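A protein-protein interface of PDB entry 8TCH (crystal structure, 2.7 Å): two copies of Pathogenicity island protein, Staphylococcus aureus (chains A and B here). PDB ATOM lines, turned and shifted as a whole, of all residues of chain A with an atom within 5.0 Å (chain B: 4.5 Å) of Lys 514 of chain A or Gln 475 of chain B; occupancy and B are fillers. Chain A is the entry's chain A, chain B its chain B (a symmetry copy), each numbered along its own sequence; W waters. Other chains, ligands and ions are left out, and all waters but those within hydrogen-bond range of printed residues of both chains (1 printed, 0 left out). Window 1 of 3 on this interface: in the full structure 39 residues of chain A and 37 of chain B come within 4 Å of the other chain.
NZ of Lys 514 of chain A lies within salt-bridge range of OE2 of Glu 511 of chain A, at 2.7 Å.
The side-chain amino group (NZ) of Lys 514 of chain A lies within hydrogen-bond range of the side-chain amide oxygen (OE1) of Gln 475 of chain B (2.9 Å).
The side-chain amide nitrogen (NE2) of Gln 543 of chain A lies close to the side-chain amide nitrogen (NE2) of Gln 475 of chain B (3.4 Å).
Water W1 lies within hydrogen-bond range of O of Gln 475 of chain B (2.8 Å), N of Glu 511 of chain A (2.9 Å) and N of Gly 510 of chain A (3.5 Å).
Among the printed residues, merely in contact across the chains: Gly 510 of chain A with Gln 475 of chain B (3.3 Å), Glu 511 of chain A with Gln 475 of chain B (3.5 Å), Glu 511 of chain A with Tyr 476 of chain B (3.2 Å) and Lys 514 of chain A with Glu 472 of chain B (3.7 Å).
Lys 514 of chain A touches two residues of chain B.
Gln 475 of chain B touches four residues of chain A.
Printed residues of chain B within 4 Å of Gly 510 of chain A: Gln 475 (3.3 Å).
Printed residues of chain B within 4 Å of Gln 543 of chain A: Gln 475.
Printed residues of chain A within 4 Å of Glu 472 of chain B: Lys 514 (3.7 Å).
Of the printed residues of chain A, Tyr 476 of chain B touches Glu 511.
Thr 512 of chain A touches none of the printed residues of chain B.
Leu 521 of chain A touches none of the printed residues of chain B.
The nearest printed residue of chain B that does not touch Lys 514 of chain A is Tyr 476 of chain B (4.8 Å).
No position is printed for both chains.
Of the 6 pairs that touch across the chains among the printed residues, none has its exchanged pair printed and touching as well.
Hydrophobic or aromatic side chains of chain B that line the printed part of chain A: Tyr 476.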
ATOM      1  N   GLY A 510     -27.716 -23.484 -22.565  1.00  0.00           N
ATOM      2  CA  GLY A 510     -27.382 -24.469 -23.578  1.00  0.00           C
ATOM      3  C   GLY A 510     -26.373 -23.966 -24.588  1.00  0.00           C
ATOM      4  O   GLY A 510     -25.488 -24.710 -25.017  1.00  0.00           O
ATOM      5  N   GLU A 511     -26.489 -22.696 -24.984  1.00  0.00           N
ATOM      6  CA  GLU A 511     -25.625 -22.170 -26.035  1.00  0.00           C
ATOM      7  C   GLU A 511     -24.163 -22.155 -25.601  1.00  0.00           C
ATOM      8  O   GLU A 511     -23.270 -22.434 -26.409  1.00  0.00           O
ATOM      9  CB  GLU A 511     -26.076 -20.767 -26.439  1.00  0.00           C
ATOM     10  CG  GLU A 511     -25.209 -20.119 -27.506  1.00  0.00           C
ATOM     11  CD  GLU A 511     -25.381 -20.750 -28.875  1.00  0.00           C
ATOM     12  OE1 GLU A 511     -24.631 -20.370 -29.801  1.00  0.00           O
ATOM     13  OE2 GLU A 511     -26.260 -21.625 -29.031  1.00  0.00           O
ATOM     14  N   THR A 512     -23.892 -21.816 -24.336  1.00  0.00           N
ATOM     15  CA  THR A 512     -22.513 -21.827 -23.852  1.00  0.00           C
ATOM     16  C   THR A 512     -21.961 -23.247 -23.805  1.00  0.00           C
ATOM     17  O   THR A 512     -20.799 -23.491 -24.169  1.00  0.00           O
ATOM     18  CB  THR A 512     -22.438 -21.172 -22.472  1.00  0.00           C
ATOM     19  OG1 THR A 512     -22.568 -19.750 -22.607  1.00  0.00           O
ATOM     20  CG2 THR A 512     -21.126 -21.489 -21.777  1.00  0.00           C
ATOM     21  N   VAL A 513     -22.790 -24.206 -23.392  1.00  0.00           N
ATOM     22  CA  VAL A 513     -22.343 -25.595 -23.369  1.00  0.00           C
ATOM     23  C   VAL A 513     -22.052 -26.080 -24.782  1.00  0.00           C
ATOM     24  O   VAL A 513     -21.121 -26.862 -25.002  1.00  0.00           O
ATOM     25  CB  VAL A 513     -23.382 -26.487 -22.665  1.00  0.00           C
ATOM     26  CG1 VAL A 513     -22.888 -27.924 -22.617  1.00  0.00           C
ATOM     27  CG2 VAL A 513     -23.656 -25.964 -21.261  1.00  0.00           C
ATOM     28  N   LYS A 514     -22.840 -25.629 -25.765  1.00  0.00           N
ATOM     29  CA  LYS A 514     -22.538 -25.980 -27.150  1.00  0.00           C
ATOM     30  C   LYS A 514     -21.232 -25.332 -27.590  1.00  0.00           C
ATOM     31  O   LYS A 514     -20.359 -26.001 -28.150  1.00  0.00           O
ATOM     32  CB  LYS A 514     -23.684 -25.581 -28.076  1.00  0.00           C
ATOM     33  CG  LYS A 514     -23.494 -26.029 -29.535  1.00  0.00           C
ATOM     34  CD  LYS A 514     -24.766 -25.764 -30.334  1.00  0.00           C
ATOM     35  CE  LYS A 514     -24.958 -24.280 -30.628  1.00  0.00           C
ATOM     36  NZ  LYS A 514     -26.400 -23.879 -30.575  1.00  0.00           N
ATOM     37  N   GLU A 515     -21.074 -24.031 -27.325  1.00  0.00           N
ATOM     38  CA  GLU A 515     -19.834 -23.345 -27.667  1.00  0.00           C
ATOM     39  C   GLU A 515     -18.622 -24.058 -27.086  1.00  0.00           C
ATOM     40  O   GLU A 515     -17.516 -23.954 -27.632  1.00  0.00           O
ATOM     41  CB  GLU A 515     -19.870 -21.896 -27.167  1.00  0.00           C
ATOM     42  CG  GLU A 515     -20.596 -20.921 -28.083  1.00  0.00           C
ATOM     43  CD  GLU A 515     -20.980 -19.605 -27.400  1.00  0.00           C
ATOM     44  OE1 GLU A 515     -20.812 -19.475 -26.167  1.00  0.00           O
ATOM     45  OE2 GLU A 515     -21.462 -18.697 -28.109  1.00  0.00           O
ATOM     46  N   LYS A 516     -18.800 -24.775 -25.978  1.00  0.00           N
ATOM     47  CA  LYS A 516     -17.668 -25.490 -25.398  1.00  0.00           C
ATOM     48  C   LYS A 516     -17.493 -26.893 -25.982  1.00  0.00           C
ATOM     49  O   LYS A 516     -16.374 -27.281 -26.334  1.00  0.00           O
ATOM     50  CB  LYS A 516     -17.814 -25.578 -23.877  1.00  0.00           C
ATOM     51  CG  LYS A 516     -16.679 -26.333 -23.186  1.00  0.00           C
ATOM     52  CD  LYS A 516     -15.395 -25.510 -23.170  1.00  0.00           C
ATOM     53  CE  LYS A 516     -14.197 -26.338 -22.735  1.00  0.00           C
ATOM     54  NZ  LYS A 516     -13.096 -25.474 -22.231  1.00  0.00           N
ATOM     55  N   LEU A 517     -18.573 -27.670 -26.089  1.00  0.00           N
ATOM     56  CA  LEU A 517     -18.442 -29.087 -26.407  1.00  0.00           C
ATOM     57  C   LEU A 517     -18.566 -29.406 -27.895  1.00  0.00           C
ATOM     58  O   LEU A 517     -18.077 -30.457 -28.321  1.00  0.00           O
ATOM     59  CB  LEU A 517     -19.480 -29.900 -25.621  1.00  0.00           C
ATOM     60  CG  LEU A 517     -19.466 -29.711 -24.103  1.00  0.00           C
ATOM     61  CD1 LEU A 517     -20.536 -30.569 -23.437  1.00  0.00           C
ATOM     62  CD2 LEU A 517     -18.098 -30.022 -23.509  1.00  0.00           C
ATOM     63  N   THR A 518     -19.202 -28.550 -28.697  1.00  0.00           N
ATOM     64  CA  THR A 518     -19.240 -28.701 -30.156  1.00  0.00           C
ATOM     65  C   THR A 518     -19.890 -30.034 -30.499  1.00  0.00           C
ATOM     66  O   THR A 518     -21.069 -30.222 -30.152  1.00  0.00           O
ATOM     67  CB  THR A 518     -17.813 -28.481 -30.676  1.00  0.00           C
ATOM     68  OG1 THR A 518     -17.404 -27.141 -30.371  1.00  0.00           O
ATOM     69  CG2 THR A 518     -17.712 -28.702 -32.179  1.00  0.00           C
ATOM     70  N   LEU A 521     -21.163 -32.678 -27.556  1.00  0.00           N
ATOM     71  CA  LEU A 521     -22.149 -32.204 -26.594  1.00  0.00           C
ATOM     72  C   LEU A 521     -22.960 -33.363 -26.044  1.00  0.00           C
ATOM     73  O   LEU A 521     -23.099 -33.522 -24.824  1.00  0.00           O
ATOM     74  CB  LEU A 521     -23.064 -31.171 -27.259  1.00  0.00           C
ATOM     75  CG  LEU A 521     -24.354 -30.768 -26.543  1.00  0.00           C
ATOM     76  CD1 LEU A 521     -24.049 -29.917 -25.326  1.00  0.00           C
ATOM     77  CD2 LEU A 521     -25.303 -30.026 -27.483  1.00  0.00           C
ATOM     78  N   GLN A 543     -31.434 -30.540 -19.853  1.00  0.00           N
ATOM     79  CA  GLN A 543     -31.508 -29.112 -19.569  1.00  0.00           C
ATOM     80  C   GLN A 543     -32.772 -28.781 -18.782  1.00  0.00           C
ATOM     81  O   GLN A 543     -33.886 -29.098 -19.214  1.00  0.00           O
ATOM     82  CB  GLN A 543     -31.467 -28.316 -20.869  1.00  0.00           C
ATOM     83  CG  GLN A 543     -30.222 -28.570 -21.690  1.00  0.00           C
ATOM     84  CD  GLN A 543     -30.016 -27.538 -22.772  1.00  0.00           C
ATOM     85  OE1 GLN A 543     -30.023 -26.335 -22.510  1.00  0.00           O
ATOM     86  NE2 GLN A 543     -29.843 -28.001 -24.004  1.00  0.00           N
ATOM     87  N   GLU B 471     -33.812 -26.136 -33.206  1.00  0.00           N
ATOM     88  CA  GLU B 471     -33.575 -26.073 -31.773  1.00  0.00           C
ATOM     89  C   GLU B 471     -32.294 -25.307 -31.482  1.00  0.00           C
ATOM     90  O   GLU B 471     -32.275 -24.410 -30.628  1.00  0.00           O
ATOM     91  CB  GLU B 471     -33.530 -27.476 -31.183  1.00  0.00           C
ATOM     92  CG  GLU B 471     -33.138 -27.519 -29.720  1.00  0.00           C
ATOM     93  CD  GLU B 471     -33.482 -28.843 -29.074  1.00  0.00           C
ATOM     94  OE1 GLU B 471     -33.970 -29.745 -29.791  1.00  0.00           O
ATOM     95  OE2 GLU B 471     -33.261 -28.983 -27.856  1.00  0.00           O
ATOM     96  N   GLU B 472     -31.226 -25.600 -32.226  1.00  0.00           N
ATOM     97  CA  GLU B 472     -29.971 -24.903 -31.989  1.00  0.00           C
ATOM     98  C   GLU B 472     -30.178 -23.401 -32.108  1.00  0.00           C
ATOM     99  O   GLU B 472     -29.822 -22.635 -31.205  1.00  0.00           O
ATOM    100  CB  GLU B 472     -28.902 -25.392 -32.962  1.00  0.00           C
ATOM    101  CG  GLU B 472     -28.404 -26.798 -32.671  1.00  0.00           C
ATOM    102  CD  GLU B 472     -27.406 -27.296 -33.702  1.00  0.00           C
ATOM    103  OE1 GLU B 472     -27.127 -26.553 -34.670  1.00  0.00           O
ATOM    104  OE2 GLU B 472     -26.905 -28.429 -33.546  1.00  0.00           O
ATOM    105  N   LEU B 473     -30.867 -22.975 -33.172  1.00  0.00           N
ATOM    106  CA  LEU B 473     -31.104 -21.548 -33.359  1.00  0.00           C
ATOM    107  C   LEU B 473     -31.829 -20.988 -32.149  1.00  0.00           C
ATOM    108  O   LEU B 473     -31.405 -19.986 -31.560  1.00  0.00           O
ATOM    109  CB  LEU B 473     -31.904 -21.310 -34.633  1.00  0.00           C
ATOM    110  CG  LEU B 473     -32.046 -19.859 -35.100  1.00  0.00           C
ATOM    111  CD1 LEU B 473     -30.754 -19.076 -34.921  1.00  0.00           C
ATOM    112  CD2 LEU B 473     -32.497 -19.821 -36.558  1.00  0.00           C
ATOM    113  N   LEU B 474     -32.896 -21.666 -31.721  1.00  0.00           N
ATOM    114  CA  LEU B 474     -33.639 -21.188 -30.564  1.00  0.00           C
ATOM    115  C   LEU B 474     -32.721 -21.134 -29.351  1.00  0.00           C
ATOM    116  O   LEU B 474     -32.653 -20.115 -28.654  1.00  0.00           O
ATOM    117  CB  LEU B 474     -34.851 -22.086 -30.322  1.00  0.00           C
ATOM    118  CG  LEU B 474     -35.865 -22.064 -31.472  1.00  0.00           C
ATOM    119  CD1 LEU B 474     -37.052 -22.971 -31.182  1.00  0.00           C
ATOM    120  CD2 LEU B 474     -36.335 -20.642 -31.755  1.00  0.00           C
ATOM    121  N   GLN B 475     -31.958 -22.205 -29.126  1.00  0.00           N
ATOM    122  CA  GLN B 475     -30.981 -22.207 -28.045  1.00  0.00           C
ATOM    123  C   GLN B 475     -30.152 -20.929 -28.099  1.00  0.00           C
ATOM    124  O   GLN B 475     -30.054 -20.183 -27.114  1.00  0.00           O
ATOM    125  CB  GLN B 475     -30.105 -23.453 -28.167  1.00  0.00           C
ATOM    126  CG  GLN B 475     -29.218 -23.752 -26.981  1.00  0.00           C
ATOM    127  CD  GLN B 475     -28.366 -24.980 -27.226  1.00  0.00           C
ATOM    128  OE1 GLN B 475     -27.612 -25.042 -28.197  1.00  0.00           O
ATOM    129  NE2 GLN B 475     -28.486 -25.970 -26.348  1.00  0.00           N
ATOM    130  N   TYR B 476     -29.626 -20.621 -29.284  1.00  0.00           N
ATOM    131  CA  TYR B 476     -28.815 -19.423 -29.452  1.00  0.00           C
ATOM    132  C   TYR B 476     -29.598 -18.176 -29.062  1.00  0.00           C
ATOM    133  O   TYR B 476     -29.135 -17.366 -28.250  1.00  0.00           O
ATOM    134  CB  TYR B 476     -28.314 -19.351 -30.897  1.00  0.00           C
ATOM    135  CG  TYR B 476     -27.607 -18.071 -31.256  1.00  0.00           C
ATOM    136  CD1 TYR B 476     -26.333 -17.808 -30.789  1.00  0.00           C
ATOM    137  CD2 TYR B 476     -28.208 -17.139 -32.088  1.00  0.00           C
ATOM    138  CE1 TYR B 476     -25.684 -16.640 -31.117  1.00  0.00           C
ATOM    139  CE2 TYR B 476     -27.565 -15.970 -32.425  1.00  0.00           C
ATOM    140  CZ  TYR B 476     -26.303 -15.728 -31.939  1.00  0.00           C
ATOM    141  OH  TYR B 476     -25.653 -14.566 -32.270  1.00  0.00           O
ATOM    142  N   LEU B 477     -30.804 -18.017 -29.613  1.00  0.00           N
ATOM    143  CA  LEU B 477     -31.581 -16.826 -29.297  1.00  0.00           C
ATOM    144  C   LEU B 477     -31.908 -16.755 -27.813  1.00  0.00           C
ATOM    145  O   LEU B 477     -32.023 -15.655 -27.260  1.00  0.00           O
ATOM    146  CB  LEU B 477     -32.861 -16.785 -30.128  1.00  0.00           C
ATOM    147  CG  LEU B 477     -32.635 -16.699 -31.639  1.00  0.00           C
ATOM    148  CD1 LEU B 477     -33.958 -16.760 -32.381  1.00  0.00           C
ATOM    149  CD2 LEU B 477     -31.865 -15.436 -32.017  1.00  0.00           C
ATOM    150  N   ASP B 478     -32.048 -17.908 -27.145  1.00  0.00           N
ATOM    151  CA  ASP B 478     -32.357 -17.868 -25.719  1.00  0.00           C
ATOM    152  C   ASP B 478     -31.280 -17.108 -24.957  1.00  0.00           C
ATOM    153  O   ASP B 478     -31.561 -16.512 -23.909  1.00  0.00           O
ATOM    154  CB  ASP B 478     -32.516 -19.284 -25.172  1.00  0.00           C
ATOM    155  CG  ASP B 478     -33.325 -19.323 -23.886  1.00  0.00           C
ATOM    156  OD1 ASP B 478     -34.039 -18.343 -23.599  1.00  0.00           O
ATOM    157  OD2 ASP B 478     -33.245 -20.341 -23.165  1.00  0.00           O
ATOM    158  N   ALA B 479     -30.055 -17.093 -25.476  1.00  0.00           N
ATOM    159  CA  ALA B 479     -28.942 -16.457 -24.790  1.00  0.00           C
ATOM    160  C   ALA B 479     -28.676 -15.042 -25.273  1.00  0.00           C
ATOM    161  O   ALA B 479     -27.742 -14.401 -24.778  1.00  0.00           O
ATOM    162  CB  ALA B 479     -27.666 -17.292 -24.962  1.00  0.00           C
ATOM    163  N   PHE B 568     -38.710 -24.040 -25.131  1.00  0.00           N
ATOM    164  CA  PHE B 568     -38.362 -22.634 -25.023  1.00  0.00           C
ATOM    165  C   PHE B 568     -39.581 -21.788 -24.686  1.00  0.00           C
ATOM    166  O   PHE B 568     -40.726 -22.161 -24.956  1.00  0.00           O
ATOM    167  CB  PHE B 568     -37.713 -22.128 -26.318  1.00  0.00           C
ATOM    168  CG  PHE B 568     -36.362 -22.726 -26.584  1.00  0.00           C
ATOM    169  CD1 PHE B 568     -35.263 -22.326 -25.841  1.00  0.00           C
ATOM    170  CD2 PHE B 568     -36.190 -23.683 -27.567  1.00  0.00           C
ATOM    171  CE1 PHE B 568     -34.015 -22.871 -26.077  1.00  0.00           C
ATOM    172  CE2 PHE B 568     -34.942 -24.231 -27.806  1.00  0.00           C
ATOM    173  CZ  PHE B 568     -33.853 -23.822 -27.060  1.00  0.00           C
HETATM  174  O   HOH W   1     -28.883 -21.072 -24.760  1.00  0.00           O
